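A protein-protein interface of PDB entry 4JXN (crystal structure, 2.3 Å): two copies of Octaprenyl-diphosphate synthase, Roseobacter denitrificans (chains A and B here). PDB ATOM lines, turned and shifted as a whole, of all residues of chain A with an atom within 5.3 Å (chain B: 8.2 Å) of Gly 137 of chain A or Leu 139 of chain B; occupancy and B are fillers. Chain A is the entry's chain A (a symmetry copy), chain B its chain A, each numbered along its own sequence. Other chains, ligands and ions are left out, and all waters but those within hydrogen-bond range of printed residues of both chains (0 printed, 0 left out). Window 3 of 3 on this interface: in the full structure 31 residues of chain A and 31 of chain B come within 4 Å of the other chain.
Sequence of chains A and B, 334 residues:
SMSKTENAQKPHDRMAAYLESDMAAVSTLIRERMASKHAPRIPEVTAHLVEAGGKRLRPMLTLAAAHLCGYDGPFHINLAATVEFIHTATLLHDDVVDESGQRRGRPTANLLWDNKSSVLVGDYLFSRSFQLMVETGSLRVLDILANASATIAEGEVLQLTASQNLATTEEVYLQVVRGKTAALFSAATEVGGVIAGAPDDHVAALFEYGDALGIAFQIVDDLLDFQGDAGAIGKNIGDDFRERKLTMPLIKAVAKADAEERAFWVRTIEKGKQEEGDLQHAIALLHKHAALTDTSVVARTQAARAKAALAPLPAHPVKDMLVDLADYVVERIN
OD2 of Asp 143 of chain B is in hydrogen-bond range of ND2 of Asn 147 of chain B (3.3 Å).
Leu 142 of chain B touches Val 134 of chain A. Asp 143 of chain B touches Val 134 of chain A. Leu 139 of chain B touches Gly 137 of chain A (CD1 to O, 3.6 Å). Leu 139 of chain A touches Gly 137 of chain B (CD1 to O, 3.6 Å). Leu 139 of chain B touches Leu 139 of chain A (CD2 to CD2, 3.5 Å). Leu 139 of chain A touches Leu 142 of chain B (CD2 to CD1, 3.8 Å). CG2 of Val 134 of chain B touches CB of Leu 142 of chain A, 3.9 Å away. CD2 of Leu 139 of chain B touches CD1 of Leu 142 of chain A (3.8 Å).
Of chain B, only Leu 139 (3.6 Å) comes within 4 Å of Gly 137 of chain A. Of chain A, only Gly 137 (3.6 Å), Leu 139 (3.5 Å) and Leu 142 (3.8 Å) come within 4 Å of Leu 139 of chain B. Of the printed residues of chain A, Val 134 of chain B touches Leu 142 (3.9 Å). Printed residues of chain A within 4 Å of Leu 142 of chain B: Val 134 and Leu 139. Arg 140 of chain B touches none of the printed residues of chain A. The nearest residue of chain B that does not touch Gly 137 of chain A is Gly 137 of chain B (8.0 Å).
Of the 8 printed residues of chain A, 4 touch a printed residue of chain B. Of the 16 printed residues of chain B, 5 touch a printed residue of chain A. Among the printed residues, 8 pairs touch across the chains.
Val 134 of chain A touches Leu 142 of chain B, and with the chains exchanged Leu 142 of chain A touches Val 134 of chain B. Gly 137 of chain A touches Leu 139 of chain B, and with the chains exchanged Leu 139 of chain A touches Gly 137 of chain B. Leu 139 of chain B touches its own counterpart, Leu 139 of chain A. Leu 139 of chain A touches Leu 142 of chain B, and with the chains exchanged Leu 142 of chain A touches Leu 139 of chain B. 7 positions are printed for both chains.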
ATOM      1  N   MET A 133      18.861 -15.860  21.818  1.00  0.00           N
ATOM      2  CA  MET A 133      19.062 -16.754  22.977  1.00  0.00           C
ATOM      3  C   MET A 133      18.358 -18.094  22.766  1.00  0.00           C
ATOM      4  O   MET A 133      18.876 -19.144  23.155  1.00  0.00           O
ATOM      5  CB  MET A 133      18.571 -16.156  24.309  1.00  0.00           C
ATOM      6  CG  MET A 133      18.178 -14.690  24.314  1.00  0.00           C
ATOM      7  SD  MET A 133      17.588 -14.175  25.946  1.00  0.00           S
ATOM      8  CE  MET A 133      16.753 -12.633  25.547  1.00  0.00           C
ATOM      9  N   VAL A 134      17.162 -18.058  22.186  1.00  0.00           N
ATOM     10  CA  VAL A 134      16.387 -19.288  21.969  1.00  0.00           C
ATOM     11  C   VAL A 134      17.155 -20.233  21.055  1.00  0.00           C
ATOM     12  O   VAL A 134      17.185 -21.449  21.279  1.00  0.00           O
ATOM     13  CB  VAL A 134      14.985 -19.001  21.367  1.00  0.00           C
ATOM     14  CG1 VAL A 134      14.337 -20.281  20.835  1.00  0.00           C
ATOM     15  CG2 VAL A 134      14.084 -18.354  22.406  1.00  0.00           C
ATOM     16  N   GLU A 135      17.781 -19.667  20.027  1.00  0.00           N
ATOM     17  CA  GLU A 135      18.580 -20.463  19.099  1.00  0.00           C
ATOM     18  C   GLU A 135      19.734 -21.228  19.759  1.00  0.00           C
ATOM     19  O   GLU A 135      20.244 -22.180  19.172  1.00  0.00           O
ATOM     20  CB  GLU A 135      19.112 -19.577  17.971  1.00  0.00           C
ATOM     21  CG  GLU A 135      18.030 -19.124  16.998  1.00  0.00           C
ATOM     22  CD  GLU A 135      18.386 -17.843  16.267  1.00  0.00           C
ATOM     23  OE1 GLU A 135      17.469 -17.034  16.007  1.00  0.00           O
ATOM     24  OE2 GLU A 135      19.577 -17.639  15.951  1.00  0.00           O
ATOM     25  N   THR A 136      20.137 -20.831  20.969  1.00  0.00           N
ATOM     26  CA  THR A 136      21.267 -21.477  21.662  1.00  0.00           C
ATOM     27  C   THR A 136      20.884 -22.810  22.259  1.00  0.00           C
ATOM     28  O   THR A 136      21.751 -23.574  22.669  1.00  0.00           O
ATOM     29  CB  THR A 136      21.852 -20.593  22.799  1.00  0.00           C
ATOM     30  OG1 THR A 136      20.908 -20.453  23.869  1.00  0.00           O
ATOM     31  CG2 THR A 136      22.217 -19.226  22.277  1.00  0.00           C
ATOM     32  N   GLY A 137      19.581 -23.056  22.366  1.00  0.00           N
ATOM     33  CA  GLY A 137      19.068 -24.295  22.943  1.00  0.00           C
ATOM     34  C   GLY A 137      19.146 -24.435  24.454  1.00  0.00           C
ATOM     35  O   GLY A 137      18.806 -25.499  24.991  1.00  0.00           O
ATOM     36  N   SER A 138      19.572 -23.380  25.155  1.00  0.00           N
ATOM     37  CA  SER A 138      19.826 -23.477  26.598  1.00  0.00           C
ATOM     38  C   SER A 138      18.772 -22.750  27.416  1.00  0.00           C
ATOM     39  O   SER A 138      18.648 -21.514  27.374  1.00  0.00           O
ATOM     40  CB  SER A 138      21.225 -22.954  26.949  1.00  0.00           C
ATOM     41  OG  SER A 138      21.406 -22.910  28.362  1.00  0.00           O
ATOM     42  N   LEU A 139      18.017 -23.530  28.177  1.00  0.00           N
ATOM     43  CA  LEU A 139      16.958 -22.966  28.985  1.00  0.00           C
ATOM     44  C   LEU A 139      17.566 -22.201  30.156  1.00  0.00           C
ATOM     45  O   LEU A 139      17.073 -21.126  30.528  1.00  0.00           O
ATOM     46  CB  LEU A 139      16.004 -24.060  29.439  1.00  0.00           C
ATOM     47  CG  LEU A 139      15.217 -24.657  28.269  1.00  0.00           C
ATOM     48  CD1 LEU A 139      14.781 -26.089  28.566  1.00  0.00           C
ATOM     49  CD2 LEU A 139      14.020 -23.777  27.937  1.00  0.00           C
ATOM     50  N   LEU A 142      18.483 -18.739  29.261  1.00  0.00           N
ATOM     51  CA  LEU A 142      17.227 -18.043  29.011  1.00  0.00           C
ATOM     52  C   LEU A 142      16.649 -17.616  30.330  1.00  0.00           C
ATOM     53  O   LEU A 142      16.194 -16.477  30.482  1.00  0.00           O
ATOM     54  CB  LEU A 142      16.236 -18.953  28.271  1.00  0.00           C
ATOM     55  CG  LEU A 142      16.496 -19.031  26.762  1.00  0.00           C
ATOM     56  CD1 LEU A 142      15.980 -20.321  26.136  1.00  0.00           C
ATOM     57  CD2 LEU A 142      15.881 -17.810  26.086  1.00  0.00           C
ATOM     58  N   MET B 133       7.197 -18.077  30.017  1.00  0.00           N
ATOM     59  CA  MET B 133       7.422 -19.076  28.952  1.00  0.00           C
ATOM     60  C   MET B 133       8.626 -19.960  29.274  1.00  0.00           C
ATOM     61  O   MET B 133       8.615 -21.162  28.997  1.00  0.00           O
ATOM     62  CB  MET B 133       7.638 -18.455  27.560  1.00  0.00           C
ATOM     63  CG  MET B 133       7.367 -16.969  27.408  1.00  0.00           C
ATOM     64  SD  MET B 133       7.716 -16.408  25.723  1.00  0.00           S
ATOM     65  CE  MET B 133       7.802 -14.627  25.956  1.00  0.00           C
ATOM     66  N   VAL B 134       9.680 -19.362  29.823  1.00  0.00           N
ATOM     67  CA  VAL B 134      10.900 -20.116  30.138  1.00  0.00           C
ATOM     68  C   VAL B 134      10.592 -21.207  31.155  1.00  0.00           C
ATOM     69  O   VAL B 134      11.088 -22.334  31.047  1.00  0.00           O
ATOM     70  CB  VAL B 134      12.032 -19.202  30.681  1.00  0.00           C
ATOM     71  CG1 VAL B 134      13.154 -20.025  31.318  1.00  0.00           C
ATOM     72  CG2 VAL B 134      12.592 -18.333  29.566  1.00  0.00           C
ATOM     73  N   THR B 136       8.150 -23.011  31.361  1.00  0.00           N
ATOM     74  CA  THR B 136       7.420 -24.140  30.756  1.00  0.00           C
ATOM     75  C   THR B 136       8.347 -25.232  30.279  1.00  0.00           C
ATOM     76  O   THR B 136       7.900 -26.328  29.962  1.00  0.00           O
ATOM     77  CB  THR B 136       6.537 -23.703  29.553  1.00  0.00           C
ATOM     78  OG1 THR B 136       7.354 -23.275  28.455  1.00  0.00           O
ATOM     79  CG2 THR B 136       5.611 -22.581  29.950  1.00  0.00           C
ATOM     80  N   GLY B 137       9.632 -24.906  30.168  1.00  0.00           N
ATOM     81  CA  GLY B 137      10.638 -25.855  29.701  1.00  0.00           C
ATOM     82  C   GLY B 137      10.660 -26.158  28.211  1.00  0.00           C
ATOM     83  O   GLY B 137      11.433 -27.020  27.770  1.00  0.00           O
ATOM     84  N   SER B 138       9.839 -25.457  27.423  1.00  0.00           N
ATOM     85  CA  SER B 138       9.682 -25.790  26.002  1.00  0.00           C
ATOM     86  C   SER B 138      10.341 -24.763  25.096  1.00  0.00           C
ATOM     87  O   SER B 138       9.923 -23.595  25.017  1.00  0.00           O
ATOM     88  CB  SER B 138       8.201 -25.951  25.632  1.00  0.00           C
ATOM     89  OG  SER B 138       8.049 -26.122  24.226  1.00  0.00           O
ATOM     90  N   LEU B 139      11.373 -25.213  24.396  1.00  0.00           N
ATOM     91  CA  LEU B 139      12.106 -24.331  23.515  1.00  0.00           C
ATOM     92  C   LEU B 139      11.255 -24.013  22.292  1.00  0.00           C
ATOM     93  O   LEU B 139      11.249 -22.871  21.809  1.00  0.00           O
ATOM     94  CB  LEU B 139      13.446 -24.950  23.147  1.00  0.00           C
ATOM     95  CG  LEU B 139      14.387 -25.039  24.351  1.00  0.00           C
ATOM     96  CD1 LEU B 139      15.399 -26.168  24.182  1.00  0.00           C
ATOM     97  CD2 LEU B 139      15.086 -23.705  24.573  1.00  0.00           C
ATOM     98  N   ARG B 140      10.519 -25.022  21.828  1.00  0.00           N
ATOM     99  CA  ARG B 140       9.609 -24.862  20.698  1.00  0.00           C
ATOM    100  C   ARG B 140       8.631 -23.694  20.877  1.00  0.00           C
ATOM    101  O   ARG B 140       8.479 -22.881  19.961  1.00  0.00           O
ATOM    102  CB  ARG B 140       8.826 -26.148  20.451  1.00  0.00           C
ATOM    103  CG  ARG B 140       7.998 -26.123  19.174  1.00  0.00           C
ATOM    104  CD  ARG B 140       8.494 -27.087  18.113  1.00  0.00           C
ATOM    105  NE  ARG B 140       7.369 -27.551  17.308  1.00  0.00           N
ATOM    106  CZ  ARG B 140       6.508 -28.478  17.715  1.00  0.00           C
ATOM    107  NH1 ARG B 140       6.667 -29.045  18.897  1.00  0.00           N
ATOM    108  NH2 ARG B 140       5.502 -28.846  16.940  1.00  0.00           N
ATOM    109  N   VAL B 141       7.964 -23.604  22.037  1.00  0.00           N
ATOM    110  CA  VAL B 141       6.985 -22.505  22.255  1.00  0.00           C
ATOM    111  C   VAL B 141       7.697 -21.160  22.373  1.00  0.00           C
ATOM    112  O   VAL B 141       7.128 -20.106  22.052  1.00  0.00           O
ATOM    113  CB  VAL B 141       6.046 -22.674  23.496  1.00  0.00           C
ATOM    114  CG1 VAL B 141       5.426 -24.066  23.553  1.00  0.00           C
ATOM    115  CG2 VAL B 141       6.735 -22.320  24.803  1.00  0.00           C
ATOM    116  N   LEU B 142       8.927 -21.208  22.875  1.00  0.00           N
ATOM    117  CA  LEU B 142       9.760 -20.022  23.030  1.00  0.00           C
ATOM    118  C   LEU B 142      10.128 -19.515  21.665  1.00  0.00           C
ATOM    119  O   LEU B 142      10.055 -18.312  21.396  1.00  0.00           O
ATOM    120  CB  LEU B 142      11.028 -20.346  23.832  1.00  0.00           C
ATOM    121  CG  LEU B 142      10.795 -20.385  25.346  1.00  0.00           C
ATOM    122  CD1 LEU B 142      11.799 -21.264  26.081  1.00  0.00           C
ATOM    123  CD2 LEU B 142      10.814 -18.960  25.891  1.00  0.00           C
ATOM    124  N   ASP B 143      10.517 -20.438  20.790  1.00  0.00           N
ATOM    125  CA  ASP B 143      10.767 -20.077  19.413  1.00  0.00           C
ATOM    126  C   ASP B 143       9.529 -19.426  18.824  1.00  0.00           C
ATOM    127  O   ASP B 143       9.620 -18.372  18.210  1.00  0.00           O
ATOM    128  CB  ASP B 143      11.153 -21.283  18.567  1.00  0.00           C
ATOM    129  CG  ASP B 143      11.913 -20.895  17.300  1.00  0.00           C
ATOM    130  OD1 ASP B 143      12.927 -20.167  17.397  1.00  0.00           O
ATOM    131  OD2 ASP B 143      11.505 -21.329  16.205  1.00  0.00           O
ATOM    132  N   ILE B 144       8.382 -20.062  19.024  1.00  0.00           N
ATOM    133  CA  ILE B 144       7.129 -19.593  18.436  1.00  0.00           C
ATOM    134  C   ILE B 144       6.820 -18.174  18.912  1.00  0.00           C
ATOM    135  O   ILE B 144       6.580 -17.292  18.102  1.00  0.00           O
ATOM    136  CB  ILE B 144       5.984 -20.581  18.740  1.00  0.00           C
ATOM    137  CG1 ILE B 144       6.208 -21.869  17.921  1.00  0.00           C
ATOM    138  CG2 ILE B 144       4.628 -19.968  18.418  1.00  0.00           C
ATOM    139  CD1 ILE B 144       5.341 -23.035  18.330  1.00  0.00           C
ATOM    140  N   LEU B 145       6.887 -17.953  20.215  1.00  0.00           N
ATOM    141  CA  LEU B 145       6.626 -16.634  20.784  1.00  0.00           C
ATOM    142  C   LEU B 145       7.756 -15.627  20.541  1.00  0.00           C
ATOM    143  O   LEU B 145       7.508 -14.410  20.541  1.00  0.00           O
ATOM    144  CB  LEU B 145       6.329 -16.750  22.290  1.00  0.00           C
ATOM    145  CG  LEU B 145       4.923 -17.289  22.604  1.00  0.00           C
ATOM    146  CD1 LEU B 145       4.834 -17.708  24.062  1.00  0.00           C
ATOM    147  CD2 LEU B 145       3.828 -16.279  22.256  1.00  0.00           C
ATOM    148  N   ALA B 146       8.986 -16.113  20.356  1.00  0.00           N
ATOM    149  CA  ALA B 146      10.107 -15.219  20.015  1.00  0.00           C
ATOM    150  C   ALA B 146       9.933 -14.704  18.600  1.00  0.00           C
ATOM    151  O   ALA B 146      10.067 -13.512  18.357  1.00  0.00           O
ATOM    152  CB  ALA B 146      11.453 -15.911  20.166  1.00  0.00           C
ATOM    153  N   ASN B 147       9.607 -15.597  17.672  1.00  0.00           N
ATOM    154  CA  ASN B 147       9.352 -15.175  16.296  1.00  0.00           C
ATOM    155  C   ASN B 147       8.120 -14.307  16.151  1.00  0.00           C
ATOM    156  O   ASN B 147       8.097 -13.392  15.333  1.00  0.00           O
ATOM    157  CB  ASN B 147       9.235 -16.381  15.389  1.00  0.00           C
ATOM    158  CG  ASN B 147      10.507 -17.208  15.373  1.00  0.00           C
ATOM    159  OD1 ASN B 147      11.589 -16.711  15.700  1.00  0.00           O
ATOM    160  ND2 ASN B 147      10.386 -18.473  15.007  1.00  0.00           N
ATOM    161  N   VAL B 194       1.220 -26.985  20.912  1.00  0.00           N
ATOM    162  CA  VAL B 194       2.586 -27.476  21.068  1.00  0.00           C
ATOM    163  C   VAL B 194       2.823 -27.964  22.481  1.00  0.00           C
ATOM    164  O   VAL B 194       3.408 -29.025  22.685  1.00  0.00           O
ATOM    165  CB  VAL B 194       3.612 -26.390  20.707  1.00  0.00           C
ATOM    166  CG1 VAL B 194       5.000 -26.727  21.249  1.00  0.00           C
ATOM    167  CG2 VAL B 194       3.648 -26.201  19.199  1.00  0.00           C
ATOM    168  N   ILE B 195       2.358 -27.194  23.456  1.00  0.00           N
ATOM    169  CA  ILE B 195       2.543 -27.573  24.846  1.00  0.00           C
ATOM    170  C   ILE B 195       1.763 -28.858  25.132  1.00  0.00           C
ATOM    171  O   ILE B 195       2.190 -29.685  25.943  1.00  0.00           O
ATOM    172  CB  ILE B 195       2.158 -26.428  25.812  1.00  0.00           C
ATOM    173  CG1 ILE B 195       2.804 -26.637  27.188  1.00  0.00           C
ATOM    174  CG2 ILE B 195       0.647 -26.296  25.935  1.00  0.00           C
ATOM    175  CD1 ILE B 195       4.313 -26.504  27.191  1.00  0.00           C
